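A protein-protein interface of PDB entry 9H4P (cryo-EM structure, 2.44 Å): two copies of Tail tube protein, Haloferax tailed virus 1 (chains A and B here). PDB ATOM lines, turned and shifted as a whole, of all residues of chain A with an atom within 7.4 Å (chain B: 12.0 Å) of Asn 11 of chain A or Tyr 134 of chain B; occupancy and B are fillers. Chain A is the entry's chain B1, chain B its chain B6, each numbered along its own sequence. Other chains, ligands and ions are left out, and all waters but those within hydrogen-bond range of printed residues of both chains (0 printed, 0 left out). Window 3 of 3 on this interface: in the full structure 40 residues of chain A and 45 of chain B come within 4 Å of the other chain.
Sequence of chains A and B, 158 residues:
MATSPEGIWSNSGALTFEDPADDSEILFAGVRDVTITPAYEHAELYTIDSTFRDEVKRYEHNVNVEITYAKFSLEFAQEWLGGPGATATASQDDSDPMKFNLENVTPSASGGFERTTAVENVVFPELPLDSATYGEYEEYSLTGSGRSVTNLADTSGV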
ATOM      1  N   ILE A   8     -14.610   0.194  33.948  1.00  0.00           N
ATOM      2  CA  ILE A   8     -15.023  -1.185  33.703  1.00  0.00           C
ATOM      3  C   ILE A   8     -13.783  -1.992  33.320  1.00  0.00           C
ATOM      4  O   ILE A   8     -12.975  -1.549  32.501  1.00  0.00           O
ATOM      5  CB  ILE A   8     -16.183  -1.303  32.674  1.00  0.00           C
ATOM      6  CG1 ILE A   8     -17.422  -0.510  33.123  1.00  0.00           C
ATOM      7  CG2 ILE A   8     -16.528  -2.768  32.386  1.00  0.00           C
ATOM      8  CD1 ILE A   8     -18.671  -0.680  32.267  1.00  0.00           C
ATOM      9  N   TRP A   9     -13.655  -3.177  33.927  1.00  0.00           N
ATOM     10  CA  TRP A   9     -12.509  -4.048  33.724  1.00  0.00           C
ATOM     11  C   TRP A   9     -12.885  -5.138  32.719  1.00  0.00           C
ATOM     12  O   TRP A   9     -13.883  -5.833  32.926  1.00  0.00           O
ATOM     13  CB  TRP A   9     -12.081  -4.609  35.088  1.00  0.00           C
ATOM     14  CG  TRP A   9     -10.926  -5.562  35.043  1.00  0.00           C
ATOM     15  CD1 TRP A   9     -10.921  -6.855  35.487  1.00  0.00           C
ATOM     16  CD2 TRP A   9      -9.596  -5.302  34.541  1.00  0.00           C
ATOM     17  NE1 TRP A   9      -9.683  -7.416  35.297  1.00  0.00           N
ATOM     18  CE2 TRP A   9      -8.849  -6.495  34.710  1.00  0.00           C
ATOM     19  CE3 TRP A   9      -8.958  -4.187  33.969  1.00  0.00           C
ATOM     20  CZ2 TRP A   9      -7.505  -6.597  34.329  1.00  0.00           C
ATOM     21  CZ3 TRP A   9      -7.631  -4.290  33.592  1.00  0.00           C
ATOM     22  CH2 TRP A   9      -6.917  -5.482  33.766  1.00  0.00           C
ATOM     23  N   SER A  10     -12.099  -5.266  31.634  1.00  0.00           N
ATOM     24  CA  SER A  10     -12.451  -6.117  30.498  1.00  0.00           C
ATOM     25  C   SER A  10     -12.652  -7.580  30.906  1.00  0.00           C
ATOM     26  O   SER A  10     -13.561  -8.243  30.397  1.00  0.00           O
ATOM     27  CB  SER A  10     -11.447  -6.009  29.376  1.00  0.00           C
ATOM     28  OG  SER A  10     -11.343  -4.670  28.909  1.00  0.00           O
ATOM     29  N   ASN A  11     -11.804  -8.069  31.825  1.00  0.00           N
ATOM     30  CA  ASN A  11     -11.796  -9.471  32.229  1.00  0.00           C
ATOM     31  C   ASN A  11     -12.979  -9.829  33.143  1.00  0.00           C
ATOM     32  O   ASN A  11     -13.166 -11.011  33.448  1.00  0.00           O
ATOM     33  CB  ASN A  11     -10.453  -9.873  32.855  1.00  0.00           C
ATOM     34  CG  ASN A  11      -9.263  -9.733  31.925  1.00  0.00           C
ATOM     35  OD1 ASN A  11      -9.189  -8.807  31.113  1.00  0.00           O
ATOM     36  ND2 ASN A  11      -8.309 -10.644  32.048  1.00  0.00           N
ATOM     37  N   SER A  12     -13.774  -8.828  33.573  1.00  0.00           N
ATOM     38  CA  SER A  12     -14.980  -9.052  34.366  1.00  0.00           C
ATOM     39  C   SER A  12     -16.186  -9.410  33.486  1.00  0.00           C
ATOM     40  O   SER A  12     -17.250  -9.737  34.017  1.00  0.00           O
ATOM     41  CB  SER A  12     -15.291  -7.855  35.252  1.00  0.00           C
ATOM     42  OG  SER A  12     -14.211  -7.565  36.129  1.00  0.00           O
ATOM     43  N   GLY A  13     -16.030  -9.340  32.153  1.00  0.00           N
ATOM     44  CA  GLY A  13     -17.130  -9.550  31.221  1.00  0.00           C
ATOM     45  C   GLY A  13     -17.496 -11.024  31.034  1.00  0.00           C
ATOM     46  O   GLY A  13     -16.618 -11.887  30.995  1.00  0.00           O
ATOM     47  N   ALA A  14     -18.808 -11.280  30.905  1.00  0.00           N
ATOM     48  CA  ALA A  14     -19.347 -12.572  30.506  1.00  0.00           C
ATOM     49  C   ALA A  14     -20.200 -12.399  29.245  1.00  0.00           C
ATOM     50  O   ALA A  14     -21.245 -11.747  29.286  1.00  0.00           O
ATOM     51  CB  ALA A  14     -20.126 -13.190  31.650  1.00  0.00           C
ATOM     52  N   VAL A  31     -13.121 -15.371  25.097  1.00  0.00           N
ATOM     53  CA  VAL A  31     -12.975 -14.065  24.461  1.00  0.00           C
ATOM     54  C   VAL A  31     -11.711 -13.368  24.979  1.00  0.00           C
ATOM     55  O   VAL A  31     -11.263 -13.614  26.103  1.00  0.00           O
ATOM     56  CB  VAL A  31     -14.238 -13.181  24.603  1.00  0.00           C
ATOM     57  CG1 VAL A  31     -15.422 -13.744  23.819  1.00  0.00           C
ATOM     58  CG2 VAL A  31     -14.624 -12.897  26.057  1.00  0.00           C
ATOM     59  N   ARG A  32     -11.141 -12.509  24.118  1.00  0.00           N
ATOM     60  CA  ARG A  32      -9.946 -11.727  24.412  1.00  0.00           C
ATOM     61  C   ARG A  32     -10.179 -10.254  24.058  1.00  0.00           C
ATOM     62  O   ARG A  32      -9.582  -9.374  24.678  1.00  0.00           O
ATOM     63  CB  ARG A  32      -8.702 -12.348  23.765  1.00  0.00           C
ATOM     64  CG  ARG A  32      -8.449 -13.797  24.176  1.00  0.00           C
ATOM     65  CD  ARG A  32      -7.061 -14.328  23.869  1.00  0.00           C
ATOM     66  NE  ARG A  32      -6.080 -13.707  24.752  1.00  0.00           N
ATOM     67  CZ  ARG A  32      -5.199 -12.763  24.411  1.00  0.00           C
ATOM     68  NH1 ARG A  32      -4.373 -12.280  25.323  1.00  0.00           N
ATOM     69  NH2 ARG A  32      -5.128 -12.310  23.171  1.00  0.00           N
ATOM     70  N   ASP A  33     -11.057  -9.995  23.075  1.00  0.00           N
ATOM     71  CA  ASP A  33     -11.597  -8.661  22.838  1.00  0.00           C
ATOM     72  C   ASP A  33     -13.086  -8.756  22.492  1.00  0.00           C
ATOM     73  O   ASP A  33     -13.515  -9.727  21.862  1.00  0.00           O
ATOM     74  CB  ASP A  33     -10.860  -7.929  21.709  1.00  0.00           C
ATOM     75  CG  ASP A  33      -9.402  -7.619  21.989  1.00  0.00           C
ATOM     76  OD1 ASP A  33      -8.577  -8.547  21.895  1.00  0.00           O
ATOM     77  OD2 ASP A  33      -9.104  -6.451  22.277  1.00  0.00           O
ATOM     78  N   VAL A  34     -13.857  -7.732  22.899  1.00  0.00           N
ATOM     79  CA  VAL A  34     -15.255  -7.552  22.513  1.00  0.00           C
ATOM     80  C   VAL A  34     -15.503  -6.053  22.310  1.00  0.00           C
ATOM     81  O   VAL A  34     -15.344  -5.267  23.248  1.00  0.00           O
ATOM     82  CB  VAL A  34     -16.244  -8.132  23.557  1.00  0.00           C
ATOM     83  CG1 VAL A  34     -17.708  -7.874  23.193  1.00  0.00           C
ATOM     84  CG2 VAL A  34     -16.034  -9.617  23.861  1.00  0.00           C
ATOM     85  N   THR A 106     -21.293  -7.143  32.506  1.00  0.00           N
ATOM     86  CA  THR A 106     -20.086  -6.693  33.191  1.00  0.00           C
ATOM     87  C   THR A 106     -20.439  -5.960  34.487  1.00  0.00           C
ATOM     88  O   THR A 106     -21.239  -5.021  34.460  1.00  0.00           O
ATOM     89  CB  THR A 106     -19.278  -5.695  32.342  1.00  0.00           C
ATOM     90  OG1 THR A 106     -20.150  -4.682  31.833  1.00  0.00           O
ATOM     91  CG2 THR A 106     -18.508  -6.326  31.202  1.00  0.00           C
ATOM     92  N   PRO A 107     -19.868  -6.356  35.657  1.00  0.00           N
ATOM     93  CA  PRO A 107     -19.791  -5.459  36.819  1.00  0.00           C
ATOM     94  C   PRO A 107     -18.912  -4.246  36.498  1.00  0.00           C
ATOM     95  O   PRO A 107     -17.947  -4.361  35.735  1.00  0.00           O
ATOM     96  CB  PRO A 107     -19.109  -6.305  37.917  1.00  0.00           C
ATOM     97  CG  PRO A 107     -19.272  -7.749  37.464  1.00  0.00           C
ATOM     98  CD  PRO A 107     -19.312  -7.694  35.947  1.00  0.00           C
ATOM     99  N   GLU A 139      -6.244 -17.966  17.269  1.00  0.00           N
ATOM    100  CA  GLU A 139      -7.046 -16.815  17.671  1.00  0.00           C
ATOM    101  C   GLU A 139      -7.979 -16.430  16.519  1.00  0.00           C
ATOM    102  O   GLU A 139      -7.527 -16.236  15.389  1.00  0.00           O
ATOM    103  CB  GLU A 139      -6.131 -15.670  18.125  1.00  0.00           C
ATOM    104  CG  GLU A 139      -6.849 -14.554  18.862  1.00  0.00           C
ATOM    105  CD  GLU A 139      -5.926 -13.552  19.528  1.00  0.00           C
ATOM    106  OE1 GLU A 139      -4.992 -13.071  18.862  1.00  0.00           O
ATOM    107  OE2 GLU A 139      -6.143 -13.263  20.715  1.00  0.00           O
ATOM    108  N   ASP B 130     -19.630  -1.439  24.593  1.00  0.00           N
ATOM    109  CA  ASP B 130     -18.637  -2.346  25.140  1.00  0.00           C
ATOM    110  C   ASP B 130     -17.363  -2.216  24.306  1.00  0.00           C
ATOM    111  O   ASP B 130     -17.427  -2.167  23.076  1.00  0.00           O
ATOM    112  CB  ASP B 130     -19.169  -3.786  25.145  1.00  0.00           C
ATOM    113  CG  ASP B 130     -20.437  -4.011  25.958  1.00  0.00           C
ATOM    114  OD1 ASP B 130     -21.399  -3.233  25.791  1.00  0.00           O
ATOM    115  OD2 ASP B 130     -20.460  -4.978  26.740  1.00  0.00           O
ATOM    116  N   SER B 131     -16.213  -2.140  24.992  1.00  0.00           N
ATOM    117  CA  SER B 131     -14.921  -1.916  24.359  1.00  0.00           C
ATOM    118  C   SER B 131     -13.836  -2.625  25.171  1.00  0.00           C
ATOM    119  O   SER B 131     -12.904  -1.995  25.680  1.00  0.00           O
ATOM    120  CB  SER B 131     -14.651  -0.432  24.203  1.00  0.00           C
ATOM    121  OG  SER B 131     -13.432  -0.201  23.509  1.00  0.00           O
ATOM    122  N   ALA B 132     -13.994  -3.952  25.297  1.00  0.00           N
ATOM    123  CA  ALA B 132     -13.180  -4.784  26.172  1.00  0.00           C
ATOM    124  C   ALA B 132     -11.954  -5.314  25.423  1.00  0.00           C
ATOM    125  O   ALA B 132     -12.078  -5.852  24.321  1.00  0.00           O
ATOM    126  CB  ALA B 132     -14.024  -5.906  26.741  1.00  0.00           C
ATOM    127  N   THR B 133     -10.774  -5.135  26.038  1.00  0.00           N
ATOM    128  CA  THR B 133      -9.536  -5.777  25.613  1.00  0.00           C
ATOM    129  C   THR B 133      -8.921  -6.465  26.827  1.00  0.00           C
ATOM    130  O   THR B 133      -8.771  -5.840  27.878  1.00  0.00           O
ATOM    131  CB  THR B 133      -8.534  -4.759  25.042  1.00  0.00           C
ATOM    132  OG1 THR B 133      -9.076  -4.213  23.839  1.00  0.00           O
ATOM    133  CG2 THR B 133      -7.159  -5.332  24.754  1.00  0.00           C
ATOM    134  N   TYR B 134      -8.547  -7.738  26.651  1.00  0.00           N
ATOM    135  CA  TYR B 134      -7.981  -8.557  27.711  1.00  0.00           C
ATOM    136  C   TYR B 134      -6.808  -7.838  28.394  1.00  0.00           C
ATOM    137  O   TYR B 134      -5.884  -7.374  27.718  1.00  0.00           O
ATOM    138  CB  TYR B 134      -7.578  -9.908  27.113  1.00  0.00           C
ATOM    139  CG  TYR B 134      -6.694 -10.724  28.016  1.00  0.00           C
ATOM    140  CD1 TYR B 134      -7.260 -11.603  28.928  1.00  0.00           C
ATOM    141  CD2 TYR B 134      -5.307 -10.587  27.980  1.00  0.00           C
ATOM    142  CE1 TYR B 134      -6.460 -12.347  29.781  1.00  0.00           C
ATOM    143  CE2 TYR B 134      -4.495 -11.321  28.830  1.00  0.00           C
ATOM    144  CZ  TYR B 134      -5.081 -12.202  29.726  1.00  0.00           C
ATOM    145  OH  TYR B 134      -4.301 -12.935  30.566  1.00  0.00           O
ATOM    146  N   GLY B 135      -6.862  -7.751  29.734  1.00  0.00           N
ATOM    147  CA  GLY B 135      -5.814  -7.140  30.544  1.00  0.00           C
ATOM    148  C   GLY B 135      -5.817  -5.605  30.534  1.00  0.00           C
ATOM    149  O   GLY B 135      -4.846  -5.000  30.993  1.00  0.00           O
ATOM    150  N   GLU B 136      -6.903  -4.981  30.039  1.00  0.00           N
ATOM    151  CA  GLU B 136      -7.050  -3.526  30.041  1.00  0.00           C
ATOM    152  C   GLU B 136      -8.424  -3.136  30.593  1.00  0.00           C
ATOM    153  O   GLU B 136      -9.367  -3.921  30.504  1.00  0.00           O
ATOM    154  CB  GLU B 136      -6.895  -2.954  28.625  1.00  0.00           C
ATOM    155  CG  GLU B 136      -5.484  -3.018  28.076  1.00  0.00           C
ATOM    156  CD  GLU B 136      -5.247  -2.000  26.980  1.00  0.00           C
ATOM    157  OE1 GLU B 136      -5.662  -2.256  25.838  1.00  0.00           O
ATOM    158  OE2 GLU B 136      -4.676  -0.943  27.282  1.00  0.00           O
ATOM    159  N   TYR B 137      -8.526  -1.924  31.165  1.00  0.00           N
ATOM    160  CA  TYR B 137      -9.825  -1.305  31.401  1.00  0.00           C
ATOM    161  C   TYR B 137     -10.472  -1.012  30.049  1.00  0.00           C
ATOM    162  O   TYR B 137      -9.767  -0.765  29.067  1.00  0.00           O
ATOM    163  CB  TYR B 137      -9.698  -0.036  32.255  1.00  0.00           C
ATOM    164  CG  TYR B 137      -9.175  -0.350  33.631  1.00  0.00           C
ATOM    165  CD1 TYR B 137      -7.805  -0.408  33.868  1.00  0.00           C
ATOM    166  CD2 TYR B 137     -10.041  -0.688  34.665  1.00  0.00           C
ATOM    167  CE1 TYR B 137      -7.309  -0.756  35.115  1.00  0.00           C
ATOM    168  CE2 TYR B 137      -9.559  -1.033  35.919  1.00  0.00           C
ATOM    169  CZ  TYR B 137      -8.190  -1.066  36.141  1.00  0.00           C
ATOM    170  OH  TYR B 137      -7.711  -1.392  37.377  1.00  0.00           O
ATOM    171  N   GLU B 138     -11.808  -1.058  30.003  1.00  0.00           N
ATOM    172  CA  GLU B 138     -12.517  -0.659  28.794  1.00  0.00           C
ATOM    173  C   GLU B 138     -12.239   0.819  28.506  1.00  0.00           C
ATOM    174  O   GLU B 138     -12.289   1.651  29.417  1.00  0.00           O
ATOM    175  CB  GLU B 138     -14.025  -0.874  28.944  1.00  0.00           C
ATOM    176  CG  GLU B 138     -14.455  -2.331  29.021  1.00  0.00           C
ATOM    177  CD  GLU B 138     -15.900  -2.559  28.607  1.00  0.00           C
ATOM    178  OE1 GLU B 138     -16.404  -1.791  27.760  1.00  0.00           O
ATOM    179  OE2 GLU B 138     -16.519  -3.501  29.132  1.00  0.00           O
ATOM    180  N   GLU B 139     -11.946   1.132  27.235  1.00  0.00           N
ATOM    181  CA  GLU B 139     -11.681   2.501  26.812  1.00  0.00           C
ATOM    182  C   GLU B 139     -12.526   2.823  25.577  1.00  0.00           C
ATOM    183  O   GLU B 139     -12.597   2.023  24.642  1.00  0.00           O
ATOM    184  CB  GLU B 139     -10.178   2.710  26.589  1.00  0.00           C
ATOM    185  CG  GLU B 139      -9.750   4.169  26.586  1.00  0.00           C
ATOM    186  CD  GLU B 139      -8.311   4.364  26.153  1.00  0.00           C
ATOM    187  OE1 GLU B 139      -8.024   4.182  24.956  1.00  0.00           O
ATOM    188  OE2 GLU B 139      -7.480   4.688  27.017  1.00  0.00           O
ATOM    189  N   TYR B 140     -13.138   4.016  25.586  1.00  0.00           N
ATOM    190  CA  TYR B 140     -14.181   4.401  24.643  1.00  0.00           C
ATOM    191  C   TYR B 140     -13.728   5.633  23.862  1.00  0.00           C
ATOM    192  O   TYR B 140     -13.242   6.592  24.462  1.00  0.00           O
ATOM    193  CB  TYR B 140     -15.472   4.730  25.407  1.00  0.00           C
ATOM    194  CG  TYR B 140     -15.875   3.653  26.379  1.00  0.00           C
ATOM    195  CD1 TYR B 140     -16.407   2.456  25.914  1.00  0.00           C
ATOM    196  CD2 TYR B 140     -15.667   3.797  27.748  1.00  0.00           C
ATOM    197  CE1 TYR B 140     -16.748   1.434  26.787  1.00  0.00           C
ATOM    198  CE2 TYR B 140     -16.002   2.783  28.634  1.00  0.00           C
ATOM    199  CZ  TYR B 140     -16.541   1.601  28.149  1.00  0.00           C
ATOM    200  OH  TYR B 140     -16.887   0.615  29.028  1.00  0.00           O
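The backbone NH of Glu 138 of chain B lies within hydrogen-bond range of the backbone carbonyl oxygen of Ile 8 of chain A (2.8 Å). The side-chain hydroxyl (OG) of Ser 10 of chain A sits at hydrogen-bond distance from the backbone NH (N) of Thr 133 of chain B (3.0 Å). The side-chain hydroxyl of Ser 10 of chain A is in hydrogen-bond range of the backbone carbonyl oxygen of Glu 136 of chain B (2.6 Å). The side-chain amide oxygen (OD1) of Asn 11 of chain A is in hydrogen-bond range of the backbone NH (N) of Gly 135 of chain B, 2.9 Å away. O of Arg 32 of chain A sits at hydrogen-bond distance from N of Tyr 134 of chain B (2.8 Å). The side-chain carboxylate (OD2) of Asp 33 of chain A is in hydrogen-bond range of the side-chain hydroxyl (OG1) of Thr 133 of chain B (2.7 Å). The backbone NH (N) of Ala 132 of chain B lies within hydrogen-bond range of the backbone carbonyl oxygen (O) of Val 34 of chain A (2.8 Å).
OE2 of Glu 139 of chain A is in salt-bridge range of NH2 of Arg 32 of chain A (2.8 Å). The backbone NH (N) of Ser 131 of chain B is in hydrogen-bond range of the side-chain carboxylate (OE1) of Glu 138 of chain B, 2.8 Å away. O of Glu 139 of chain B lies within hydrogen-bond range of OG of Ser 131 of chain B (2.6 Å). The side-chain carboxylate (OE1) of Glu 138 of chain B is in hydrogen-bond range of the side-chain hydroxyl (OH) of Tyr 140 of chain B, at 2.8 Å.
Among the printed residues, merely in contact across the chains: Asp 33 of chain A with Ala 132 of chain B (3.2 Å), Ser 10 of chain A with Ala 132 of chain B (3.3 Å), Trp 9 of chain A with Glu 136 of chain B (3.3 Å), Ile 8 of chain A with Tyr 137 of chain B (3.3 Å), Asn 11 of chain A with Tyr 134 of chain B (3.4 Å), Trp 9 of chain A with Gly 135 of chain B (3.4 Å), Trp 9 of chain A with Tyr 137 of chain B (3.5 Å), Val 34 of chain A with Ser 131 of chain B (3.6 Å), Arg 32 of chain A with Thr 133 of chain B (3.7 Å), Val 34 of chain A with Asp 130 of chain B (3.7 Å), Ser 10 of chain A with Glu 138 of chain B (3.8 Å), Ile 8 of chain A with Tyr 140 of chain B (3.9 Å) and Ser 10 of chain A with Tyr 137 of chain B (3.9 Å).
Trp 9 of chain A touches just these residues of chain B: Gly 135, Glu 136 and Tyr 137. Of chain B, only Ala 132 (3.3 Å), Thr 133 (3.0 Å), Glu 136 (2.6 Å), Tyr 137 (3.9 Å) and Glu 138 (3.8 Å) come within 4 Å of Ser 10 of chain A. Asn 11 of chain A touches just these residues of chain B: Tyr 134 (3.4 Å) and Gly 135 (2.9 Å). No residue of chain B comes within 4 Å of Ser 12 of chain A. Gly 13 of chain A touches none of the printed residues of chain B. Ala 14 of chain A touches none of the printed residues of chain B. Of chain B, only Thr 133 (3.7 Å) and Tyr 134 (2.8 Å) come within 4 Å of Arg 32 of chain A. Of chain B, only Ala 132 and Thr 133 come within 4 Å of Asp 33 of chain A. Of the printed residues of chain A, Asp 130 of chain B touches Val 34. Tyr 134 of chain B touches just these residues of chain A: Asn 11 (3.4 Å) and Arg 32 (2.8 Å). Printed residues of chain A within 4 Å of Gly 135 of chain B: Trp 9 and Asn 11. Of the printed residues of chain A, Glu 136 of chain B touches Trp 9 and Ser 10. Glu 139 of chain B touches none of the printed residues of chain A. The nearest residue of chain A that does not touch Tyr 134 of chain B is Ser 10 of chain A (4.3 Å). The nearest printed residue of chain A that does not touch Ser 131 of chain B is Ser 10 of chain A (4.5 Å).
Of the 11 printed residues of chain B, 10 touch a printed residue of chain A. Printed residues of chain B that touch a printed residue of chain A: Asp 130, Ser 131, Ala 132, Thr 133, Tyr 134, Gly 135, Glu 136, Tyr 137, Glu 138 and Tyr 140. Along chain B the printed residues that touch a printed residue of chain A span positions 130 to 140. Printed residues of chain A that touch a printed residue of chain B: Ile 8, Trp 9, Ser 10, Asn 11, Arg 32, Asp 33 and Val 34. Hydrophobic or aromatic side chains of chain A within 4 Å of the printed part of chain B: Ile 8 and Trp 9. Among the printed residues, 20 pairs touch across the chains. Among the printed residues, no Asp or Glu carboxylate lies within 4 Å of a Lys or Arg side-chain nitrogen of the other chain.
Position printed for both chains: 139. Of the 20 pairs that touch across the chains among the printed residues, none has its exchanged pair printed and touching as well.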
